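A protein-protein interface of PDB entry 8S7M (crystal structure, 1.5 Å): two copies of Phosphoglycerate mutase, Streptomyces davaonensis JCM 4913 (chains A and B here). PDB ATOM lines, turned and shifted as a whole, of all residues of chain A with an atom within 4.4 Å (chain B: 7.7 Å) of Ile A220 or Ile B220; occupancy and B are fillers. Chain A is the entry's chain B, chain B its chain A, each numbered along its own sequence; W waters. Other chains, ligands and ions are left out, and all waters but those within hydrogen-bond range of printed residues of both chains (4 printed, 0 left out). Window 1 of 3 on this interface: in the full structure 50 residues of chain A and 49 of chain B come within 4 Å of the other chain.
Of the printed residues of chain B, Met A189 touches Met B198. Of the printed residues of chain B, Leu A196 touches Leu B196 (3.8 Å). Of the printed residues of chain B, Met A198 touches Met B189, Val B217, Arg B218 and Ile B220. Printed residues of chain B within 4 Å of Ser A219: Met B198, Ile B220, Gly B221 and Asp B222. Ile A220 touches just these residues of chain B: Met B198, Ser B219 and Ile B220. Leu B181 touches none of the printed residues of chain A. Of the printed residues of chain A, Leu B196 touches Leu A196. The nearest residue of chain B that does not touch Ile A220 is Arg B218 (4.5 Å).
Among the printed residues, merely in contact across the chains: Ser A219 with Ile B220 (3.1 Å), Ile A220 with Ser B219 (3.1 Å), Met A198 with Arg B218 (3.3 Å), Met A198 with Met B189 (3.3 Å), Ser A219 with Gly B221 (3.3 Å), Gly A221 with Ser B219 (3.3 Å), Met A189 with Met B198 (3.6 Å), Gly A221 with Arg B218 (3.7 Å), Ser A219 with Asp B222 (3.8 Å), Leu A196 with Leu B196 (3.8 Å), Asp A222 with Ser B219 (3.8 Å), Met A198 with Val B217 (3.8 Å), Val A217 with Met B198 (3.9 Å), Ile A220 with Met B198 (3.9 Å), Met A198 with Ile B220 (3.97 Å) and Ser A219 with Met B198 (3.98 Å).
The backbone NH (N) of Gly A221 sits at hydrogen-bond distance from the side-chain hydroxyl (OG) of Ser A206, 2.8 Å away. O of Val B207 sits at hydrogen-bond distance from N of Arg B218. N of Val A205 sits at hydrogen-bond distance from O of Asp A222. N of Gly A221 lies within hydrogen-bond range of O of Val A205 (3.4 Å). The side-chain hydroxyl (OG) of Ser B206 is in hydrogen-bond range of the backbone NH (N) of Gly B221 (2.9 Å). N of Val B205 sits at hydrogen-bond distance from O of Asp B222 (2.8 Å).
Hydrophobic or aromatic side chains of chain B within 4 Å of the printed part of chain A: Met B189, Leu B196, Met B198 and Ile B220. Among the printed residues, no Asp or Glu carboxylate lies within 4 Å of a Lys or Arg side-chain nitrogen of the other chain.
The side-chain carboxylate of Asp B222 sits close to the side-chain carboxylate of Asp A222, at 3.3 Å. The backbone NH (N) of Ile B220 is in hydrogen-bond range of the backbone carbonyl oxygen (O) of Ile A220 (2.9 Å).
Water W1 lies within hydrogen-bond range of OG of Ser A219 (2.6 Å), OD2 of Asp B222 (2.7 Å) and O of Val A205 (2.7 Å). Water W4 lies within hydrogen-bond range of OD2 of Asp A222 (2.6 Å), OG of Ser B219 (2.7 Å) and O of Val B205 (2.7 Å). Water W2 bridges OG of Ser A219 and N of Ala B223. Water W3 bridges the backbone carbonyl oxygen of Val A217 (3.1 Å) and the backbone NH of Ile B199 (3.2 Å).
Leu A196 touches its own counterpart, Leu B196. Ser A219 touches Ile B220, and with the chains exchanged Ile A220 touches Ser B219. Ile A220 touches its own counterpart, Ile B220. Asp B222 touches its own counterpart, Asp A222.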
ATOM      1  N   MET A 185       4.978  20.775  13.764  1.00  0.00           N
ATOM      2  CA  MET A 185       4.444  20.079  14.925  1.00  0.00           C
ATOM      3  C   MET A 185       3.257  20.792  15.553  1.00  0.00           C
ATOM      4  O   MET A 185       2.276  20.138  15.913  1.00  0.00           O
ATOM      5  CB  MET A 185       5.552  19.726  15.902  1.00  0.00           C
ATOM      6  CG  MET A 185       6.469  18.652  15.292  1.00  0.00           C
ATOM      7  SD  MET A 185       7.705  18.060  16.452  1.00  0.00           S
ATOM      8  CE  MET A 185       8.861  19.418  16.405  1.00  0.00           C
ATOM      9  N   MET A 189      -1.044  19.589  15.710  1.00  0.00           N
ATOM     10  CA  MET A 189      -1.907  19.625  16.882  1.00  0.00           C
ATOM     11  C   MET A 189      -2.966  20.712  16.777  1.00  0.00           C
ATOM     12  O   MET A 189      -3.585  21.064  17.786  1.00  0.00           O
ATOM     13  CB  MET A 189      -1.075  19.846  18.140  1.00  0.00           C
ATOM     14  CG  MET A 189      -0.256  18.668  18.531  1.00  0.00           C
ATOM     15  SD  MET A 189       0.689  19.137  19.999  1.00  0.00           S
ATOM     16  CE  MET A 189       2.115  18.087  19.862  1.00  0.00           C
ATOM     17  N   LEU A 196       2.182  26.160  21.004  1.00  0.00           N
ATOM     18  CA  LEU A 196       3.227  25.209  21.351  1.00  0.00           C
ATOM     19  C   LEU A 196       4.474  26.050  21.578  1.00  0.00           C
ATOM     20  O   LEU A 196       5.237  26.318  20.646  1.00  0.00           O
ATOM     21  CB  LEU A 196       3.430  24.186  20.233  1.00  0.00           C
ATOM     22  CG  LEU A 196       4.450  23.075  20.464  1.00  0.00           C
ATOM     23  CD1 LEU A 196       3.972  22.183  21.579  1.00  0.00           C
ATOM     24  CD2 LEU A 196       4.653  22.260  19.191  1.00  0.00           C
ATOM     25  N   MET A 198       7.685  26.621  22.405  1.00  0.00           N
ATOM     26  CA  MET A 198       8.979  25.962  22.530  1.00  0.00           C
ATOM     27  C   MET A 198       9.864  26.373  21.373  1.00  0.00           C
ATOM     28  O   MET A 198       9.384  26.663  20.273  1.00  0.00           O
ATOM     29  CB  MET A 198       8.872  24.431  22.421  1.00  0.00           C
ATOM     30  CG  MET A 198       7.927  23.768  23.368  1.00  0.00           C
ATOM     31  SD  MET A 198       7.841  21.993  23.071  1.00  0.00           S
ATOM     32  CE  MET A 198       9.542  21.503  23.418  1.00  0.00           C
ATOM     33  N   LEU A 200      13.162  24.524  19.369  1.00  0.00           N
ATOM     34  CA  LEU A 200      13.806  23.222  19.249  1.00  0.00           C
ATOM     35  C   LEU A 200      15.316  23.427  19.263  1.00  0.00           C
ATOM     36  O   LEU A 200      15.832  24.178  18.417  1.00  0.00           O
ATOM     37  CB  LEU A 200      13.402  22.558  17.939  1.00  0.00           C
ATOM     38  CG  LEU A 200      11.893  22.362  17.732  1.00  0.00           C
ATOM     39  CD1 LEU A 200      11.620  21.741  16.390  1.00  0.00           C
ATOM     40  CD2 LEU A 200      11.337  21.477  18.827  1.00  0.00           C
ATOM     41  N   VAL A 205      15.984  15.952  18.410  1.00  0.00           N
ATOM     42  CA  VAL A 205      15.211  14.902  17.758  1.00  0.00           C
ATOM     43  C   VAL A 205      13.765  15.028  18.211  1.00  0.00           C
ATOM     44  O   VAL A 205      13.491  15.120  19.416  1.00  0.00           O
ATOM     45  CB  VAL A 205      15.756  13.508  18.121  1.00  0.00           C
ATOM     46  CG1 VAL A 205      14.866  12.422  17.535  1.00  0.00           C
ATOM     47  CG2 VAL A 205      17.181  13.330  17.625  1.00  0.00           C
ATOM     48  N   SER A 206      12.839  15.008  17.249  1.00  0.00           N
ATOM     49  CA  SER A 206      11.406  15.000  17.494  1.00  0.00           C
ATOM     50  C   SER A 206      10.829  13.888  16.628  1.00  0.00           C
ATOM     51  O   SER A 206      11.211  13.745  15.474  1.00  0.00           O
ATOM     52  CB  SER A 206      10.742  16.336  17.116  1.00  0.00           C
ATOM     53  OG  SER A 206      11.393  17.447  17.724  1.00  0.00           O
ATOM     54  N   VAL A 217       2.224  13.695  16.449  1.00  0.00           N
ATOM     55  CA  VAL A 217       3.430  14.110  17.171  1.00  0.00           C
ATOM     56  C   VAL A 217       3.666  13.175  18.355  1.00  0.00           C
ATOM     57  O   VAL A 217       2.835  13.081  19.265  1.00  0.00           O
ATOM     58  CB  VAL A 217       3.347  15.576  17.619  1.00  0.00           C
ATOM     59  CG1 VAL A 217       4.629  15.994  18.344  1.00  0.00           C
ATOM     60  CG2 VAL A 217       3.089  16.498  16.437  1.00  0.00           C
ATOM     61  N   SER A 219       7.105  12.891  20.000  1.00  0.00           N
ATOM     62  CA  SER A 219       8.036  13.502  20.943  1.00  0.00           C
ATOM     63  C   SER A 219       8.614  14.738  20.291  1.00  0.00           C
ATOM     64  O   SER A 219       8.595  14.865  19.068  1.00  0.00           O
ATOM     65  CB  SER A 219       9.149  12.548  21.376  1.00  0.00           C
ATOM     66  OG  SER A 219       9.935  12.141  20.279  1.00  0.00           O
ATOM     67  N   ILE A 220       9.118  15.652  21.119  1.00  0.00           N
ATOM     68  CA  ILE A 220       9.472  16.996  20.661  1.00  0.00           C
ATOM     69  C   ILE A 220      10.763  17.458  21.320  1.00  0.00           C
ATOM     70  O   ILE A 220      10.844  17.535  22.550  1.00  0.00           O
ATOM     71  CB  ILE A 220       8.377  18.027  20.990  1.00  0.00           C
ATOM     72  CG1 ILE A 220       6.997  17.572  20.504  1.00  0.00           C
ATOM     73  CG2 ILE A 220       8.754  19.370  20.399  1.00  0.00           C
ATOM     74  CD1 ILE A 220       5.905  18.584  20.786  1.00  0.00           C
ATOM     75  N   GLY A 221      11.756  17.816  20.510  1.00  0.00           N
ATOM     76  CA  GLY A 221      12.817  18.720  20.936  1.00  0.00           C
ATOM     77  C   GLY A 221      13.929  18.144  21.788  1.00  0.00           C
ATOM     78  O   GLY A 221      14.609  18.901  22.488  1.00  0.00           O
ATOM     79  N   ASP A 222      14.156  16.836  21.726  1.00  0.00           N
ATOM     80  CA  ASP A 222      15.083  16.167  22.629  1.00  0.00           C
ATOM     81  C   ASP A 222      16.517  16.265  22.110  1.00  0.00           C
ATOM     82  O   ASP A 222      16.867  15.669  21.085  1.00  0.00           O
ATOM     83  CB  ASP A 222      14.630  14.724  22.827  1.00  0.00           C
ATOM     84  CG  ASP A 222      15.520  13.961  23.770  1.00  0.00           C
ATOM     85  OD1 ASP A 222      16.757  13.913  23.545  1.00  0.00           O
ATOM     86  OD2 ASP A 222      15.005  13.500  24.801  1.00  0.00           O
ATOM     87  N   LEU B  43      11.613  14.718  33.621  1.00  0.00           N
ATOM     88  CA  LEU B  43      10.345  14.085  33.964  1.00  0.00           C
ATOM     89  C   LEU B  43      10.257  12.760  33.226  1.00  0.00           C
ATOM     90  O   LEU B  43      10.275  12.731  31.990  1.00  0.00           O
ATOM     91  CB  LEU B  43       9.196  14.985  33.521  1.00  0.00           C
ATOM     92  CG  LEU B  43       9.113  16.384  34.118  1.00  0.00           C
ATOM     93  CD1 LEU B  43       8.030  17.187  33.373  1.00  0.00           C
ATOM     94  CD2 LEU B  43       8.832  16.338  35.625  1.00  0.00           C
ATOM     95  N   LEU B 181       1.918  14.142  34.180  1.00  0.00           N
ATOM     96  CA  LEU B 181       3.057  14.817  33.555  1.00  0.00           C
ATOM     97  C   LEU B 181       2.622  15.698  32.385  1.00  0.00           C
ATOM     98  O   LEU B 181       3.067  16.848  32.263  1.00  0.00           O
ATOM     99  CB  LEU B 181       4.112  13.798  33.120  1.00  0.00           C
ATOM    100  CG  LEU B 181       4.806  13.063  34.260  1.00  0.00           C
ATOM    101  CD1 LEU B 181       5.711  11.957  33.749  1.00  0.00           C
ATOM    102  CD2 LEU B 181       5.570  14.057  35.142  1.00  0.00           C
ATOM    103  N   VAL B 182       1.736  15.186  31.519  1.00  0.00           N
ATOM    104  CA  VAL B 182       1.371  15.986  30.354  1.00  0.00           C
ATOM    105  C   VAL B 182       0.449  17.129  30.776  1.00  0.00           C
ATOM    106  O   VAL B 182       0.474  18.212  30.177  1.00  0.00           O
ATOM    107  CB  VAL B 182       0.793  15.064  29.262  1.00  0.00           C
ATOM    108  CG1 VAL B 182      -0.642  14.746  29.549  1.00  0.00           C
ATOM    109  CG2 VAL B 182       0.998  15.678  27.869  1.00  0.00           C
ATOM    110  N   MET B 185       2.962  19.819  31.904  1.00  0.00           N
ATOM    111  CA  MET B 185       3.638  20.521  30.816  1.00  0.00           C
ATOM    112  C   MET B 185       2.674  21.422  30.049  1.00  0.00           C
ATOM    113  O   MET B 185       3.049  22.533  29.645  1.00  0.00           O
ATOM    114  CB  MET B 185       4.344  19.530  29.893  1.00  0.00           C
ATOM    115  CG  MET B 185       5.502  18.851  30.599  1.00  0.00           C
ATOM    116  SD  MET B 185       6.548  17.875  29.552  1.00  0.00           S
ATOM    117  CE  MET B 185       5.665  16.327  29.703  1.00  0.00           C
ATOM    118  N   GLY B 186       1.428  20.978  29.847  1.00  0.00           N
ATOM    119  CA  GLY B 186       0.440  21.862  29.242  1.00  0.00           C
ATOM    120  C   GLY B 186       0.227  23.117  30.068  1.00  0.00           C
ATOM    121  O   GLY B 186       0.231  24.232  29.538  1.00  0.00           O
ATOM    122  N   MET B 189       2.637  25.868  29.715  1.00  0.00           N
ATOM    123  CA  MET B 189       2.457  26.623  28.478  1.00  0.00           C
ATOM    124  C   MET B 189       1.134  27.362  28.439  1.00  0.00           C
ATOM    125  O   MET B 189       0.724  27.816  27.364  1.00  0.00           O
ATOM    126  CB  MET B 189       2.478  25.701  27.267  1.00  0.00           C
ATOM    127  CG  MET B 189       3.738  24.983  27.058  1.00  0.00           C
ATOM    128  SD  MET B 189       3.657  24.046  25.529  1.00  0.00           S
ATOM    129  CE  MET B 189       5.385  23.670  25.517  1.00  0.00           C
ATOM    130  N   LEU B 196      -2.127  20.546  24.080  1.00  0.00           N
ATOM    131  CA  LEU B 196      -0.905  19.763  23.893  1.00  0.00           C
ATOM    132  C   LEU B 196      -1.361  18.324  23.756  1.00  0.00           C
ATOM    133  O   LEU B 196      -1.489  17.592  24.744  1.00  0.00           O
ATOM    134  CB  LEU B 196       0.025  19.933  25.085  1.00  0.00           C
ATOM    135  CG  LEU B 196       1.389  19.246  25.047  1.00  0.00           C
ATOM    136  CD1 LEU B 196       2.207  19.807  23.909  1.00  0.00           C
ATOM    137  CD2 LEU B 196       2.111  19.442  26.377  1.00  0.00           C
ATOM    138  N   MET B 198      -0.927  14.983  23.194  1.00  0.00           N
ATOM    139  CA  MET B 198       0.082  13.936  23.169  1.00  0.00           C
ATOM    140  C   MET B 198      -0.170  12.992  24.329  1.00  0.00           C
ATOM    141  O   MET B 198      -0.649  13.408  25.389  1.00  0.00           O
ATOM    142  CB  MET B 198       1.475  14.527  23.418  1.00  0.00           C
ATOM    143  CG  MET B 198       1.959  15.375  22.280  1.00  0.00           C
ATOM    144  SD  MET B 198       3.483  16.223  22.753  1.00  0.00           S
ATOM    145  CE  MET B 198       4.677  14.886  22.573  1.00  0.00           C
ATOM    146  N   ILE B 199       0.185  11.720  24.136  1.00  0.00           N
ATOM    147  CA  ILE B 199       0.359  10.790  25.249  1.00  0.00           C
ATOM    148  C   ILE B 199       1.850  10.504  25.388  1.00  0.00           C
ATOM    149  O   ILE B 199       2.553  10.366  24.382  1.00  0.00           O
ATOM    150  CB  ILE B 199      -0.490   9.511  25.111  1.00  0.00           C
ATOM    151  CG1 ILE B 199      -0.442   8.709  26.417  1.00  0.00           C
ATOM    152  CG2 ILE B 199      -0.082   8.680  23.889  1.00  0.00           C
ATOM    153  CD1 ILE B 199      -1.576   7.704  26.586  1.00  0.00           C
ATOM    154  N   LEU B 200       2.346  10.474  26.622  1.00  0.00           N
ATOM    155  CA  LEU B 200       3.777  10.262  26.847  1.00  0.00           C
ATOM    156  C   LEU B 200       4.058   8.772  26.958  1.00  0.00           C
ATOM    157  O   LEU B 200       3.417   8.088  27.776  1.00  0.00           O
ATOM    158  CB  LEU B 200       4.225  10.923  28.146  1.00  0.00           C
ATOM    159  CG  LEU B 200       3.923  12.416  28.263  1.00  0.00           C
ATOM    160  CD1 LEU B 200       4.333  12.926  29.656  1.00  0.00           C
ATOM    161  CD2 LEU B 200       4.559  13.211  27.149  1.00  0.00           C
ATOM    162  N   PRO B 201       4.988   8.231  26.176  1.00  0.00           N
ATOM    163  CA  PRO B 201       5.273   6.795  26.264  1.00  0.00           C
ATOM    164  C   PRO B 201       5.843   6.433  27.629  1.00  0.00           C
ATOM    165  O   PRO B 201       6.448   7.253  28.315  1.00  0.00           O
ATOM    166  CB  PRO B 201       6.328   6.571  25.175  1.00  0.00           C
ATOM    167  CG  PRO B 201       6.195   7.760  24.223  1.00  0.00           C
ATOM    168  CD  PRO B 201       5.714   8.895  25.071  1.00  0.00           C
ATOM    169  N   SER B 204       9.353   7.403  28.900  1.00  0.00           N
ATOM    170  CA  SER B 204       9.774   8.581  28.141  1.00  0.00           C
ATOM    171  C   SER B 204      10.376   9.644  29.057  1.00  0.00           C
ATOM    172  O   SER B 204      10.033   9.761  30.245  1.00  0.00           O
ATOM    173  CB  SER B 204       8.635   9.210  27.334  1.00  0.00           C
ATOM    174  OG  SER B 204       7.587   9.730  28.140  1.00  0.00           O
ATOM    175  N   VAL B 205      11.272  10.435  28.469  1.00  0.00           N
ATOM    176  CA  VAL B 205      11.958  11.528  29.136  1.00  0.00           C
ATOM    177  C   VAL B 205      11.437  12.836  28.568  1.00  0.00           C
ATOM    178  O   VAL B 205      11.460  13.037  27.342  1.00  0.00           O
ATOM    179  CB  VAL B 205      13.474  11.418  28.909  1.00  0.00           C
ATOM    180  CG1 VAL B 205      14.198  12.647  29.449  1.00  0.00           C
ATOM    181  CG2 VAL B 205      13.988  10.109  29.529  1.00  0.00           C
ATOM    182  N   SER B 206      10.985  13.729  29.457  1.00  0.00           N
ATOM    183  CA  SER B 206      10.644  15.102  29.103  1.00  0.00           C
ATOM    184  C   SER B 206      11.487  16.009  29.983  1.00  0.00           C
ATOM    185  O   SER B 206      11.785  15.661  31.122  1.00  0.00           O
ATOM    186  CB  SER B 206       9.153  15.366  29.344  1.00  0.00           C
ATOM    187  OG  SER B 206       8.346  14.416  28.649  1.00  0.00           O
ATOM    188  N   VAL B 207      11.910  17.156  29.463  1.00  0.00           N
ATOM    189  CA  VAL B 207      12.856  18.015  30.175  1.00  0.00           C
ATOM    190  C   VAL B 207      12.232  19.384  30.413  1.00  0.00           C
ATOM    191  O   VAL B 207      11.703  19.997  29.476  1.00  0.00           O
ATOM    192  CB  VAL B 207      14.188  18.146  29.413  1.00  0.00           C
ATOM    193  CG1 VAL B 207      15.158  19.118  30.131  1.00  0.00           C
ATOM    194  CG2 VAL B 207      14.828  16.779  29.282  1.00  0.00           C
ATOM    195  N   LEU B 208      12.325  19.867  31.659  1.00  0.00           N
ATOM    196  CA  LEU B 208      12.074  21.265  31.989  1.00  0.00           C
ATOM    197  C   LEU B 208      13.391  21.959  32.282  1.00  0.00           C
ATOM    198  O   LEU B 208      14.270  21.394  32.944  1.00  0.00           O
ATOM    199  CB  LEU B 208      11.192  21.418  33.231  1.00  0.00           C
ATOM    200  CG  LEU B 208       9.925  20.563  33.236  1.00  0.00           C
ATOM    201  CD1 LEU B 208       9.183  20.761  34.555  1.00  0.00           C
ATOM    202  CD2 LEU B 208       9.038  20.924  32.044  1.00  0.00           C
ATOM    203  N   VAL B 217       9.350  24.437  29.233  1.00  0.00           N
ATOM    204  CA  VAL B 217       9.301  23.085  28.681  1.00  0.00           C
ATOM    205  C   VAL B 217      10.351  22.987  27.581  1.00  0.00           C
ATOM    206  O   VAL B 217      10.203  23.605  26.522  1.00  0.00           O
ATOM    207  CB  VAL B 217       7.907  22.735  28.154  1.00  0.00           C
ATOM    208  CG1 VAL B 217       7.908  21.317  27.553  1.00  0.00           C
ATOM    209  CG2 VAL B 217       6.900  22.816  29.275  1.00  0.00           C
ATOM    210  N   ARG B 218      11.412  22.207  27.825  1.00  0.00           N
ATOM    211  CA  ARG B 218      12.530  22.052  26.892  1.00  0.00           C
ATOM    212  C   ARG B 218      12.287  20.949  25.859  1.00  0.00           C
ATOM    213  O   ARG B 218      12.589  21.142  24.674  1.00  0.00           O
ATOM    214  CB  ARG B 218      13.795  21.751  27.703  1.00  0.00           C
ATOM    215  CG  ARG B 218      15.007  21.256  26.901  1.00  0.00           C
ATOM    216  CD  ARG B 218      15.582  22.377  26.016  1.00  0.00           C
ATOM    217  NE  ARG B 218      16.228  23.398  26.834  1.00  0.00           N
ATOM    218  CZ  ARG B 218      15.793  24.646  26.974  1.00  0.00           C
ATOM    219  NH1 ARG B 218      14.722  25.087  26.312  1.00  0.00           N
ATOM    220  NH2 ARG B 218      16.449  25.473  27.795  1.00  0.00           N
ATOM    221  N   SER B 219      11.767  19.797  26.286  1.00  0.00           N
ATOM    222  CA  SER B 219      11.552  18.648  25.408  1.00  0.00           C
ATOM    223  C   SER B 219      10.475  17.754  26.007  1.00  0.00           C
ATOM    224  O   SER B 219      10.257  17.765  27.215  1.00  0.00           O
ATOM    225  CB  SER B 219      12.865  17.892  25.148  1.00  0.00           C
ATOM    226  OG  SER B 219      13.365  17.343  26.349  1.00  0.00           O
ATOM    227  N   ILE B 220       9.788  16.986  25.152  1.00  0.00           N
ATOM    228  CA  ILE B 220       8.597  16.238  25.578  1.00  0.00           C
ATOM    229  C   ILE B 220       8.587  14.828  24.998  1.00  0.00           C
ATOM    230  O   ILE B 220       8.646  14.652  23.784  1.00  0.00           O
ATOM    231  CB  ILE B 220       7.280  16.919  25.148  1.00  0.00           C
ATOM    232  CG1 ILE B 220       7.235  18.402  25.542  1.00  0.00           C
ATOM    233  CG2 ILE B 220       6.060  16.145  25.716  1.00  0.00           C
ATOM    234  CD1 ILE B 220       5.961  19.111  25.043  1.00  0.00           C
ATOM    235  N   GLY B 221       8.451  13.826  25.860  1.00  0.00           N
ATOM    236  CA  GLY B 221       7.974  12.524  25.418  1.00  0.00           C
ATOM    237  C   GLY B 221       8.954  11.603  24.722  1.00  0.00           C
ATOM    238  O   GLY B 221       8.514  10.658  24.051  1.00  0.00           O
ATOM    239  N   ASP B 222      10.260  11.809  24.891  1.00  0.00           N
ATOM    240  CA  ASP B 222      11.244  11.043  24.134  1.00  0.00           C
ATOM    241  C   ASP B 222      11.458   9.667  24.763  1.00  0.00           C
ATOM    242  O   ASP B 222      11.933   9.561  25.899  1.00  0.00           O
ATOM    243  CB  ASP B 222      12.556  11.825  24.085  1.00  0.00           C
ATOM    244  CG  ASP B 222      13.611  11.128  23.261  1.00  0.00           C
ATOM    245  OD1 ASP B 222      14.029  10.006  23.614  1.00  0.00           O
ATOM    246  OD2 ASP B 222      14.020  11.702  22.219  1.00  0.00           O
ATOM    247  N   ALA B 223      11.172   8.612  24.001  1.00  0.00           N
ATOM    248  CA  ALA B 223      11.436   7.237  24.402  1.00  0.00           C
ATOM    249  C   ALA B 223      12.295   6.549  23.355  1.00  0.00           C
ATOM    250  O   ALA B 223      12.154   5.349  23.097  1.00  0.00           O
ATOM    251  CB  ALA B 223      10.140   6.460  24.645  1.00  0.00           C
HETATM  252  O   HOH W   1      12.235  13.127  20.811  1.00  0.00           O
HETATM  253  O   HOH W   2      10.172   9.342  21.127  1.00  0.00           O
HETATM  254  O   HOH W   3       1.484  11.163  21.236  1.00  0.00           O
HETATM  255  O   HOH W   4      13.054  14.717  26.012  1.00  0.00           O
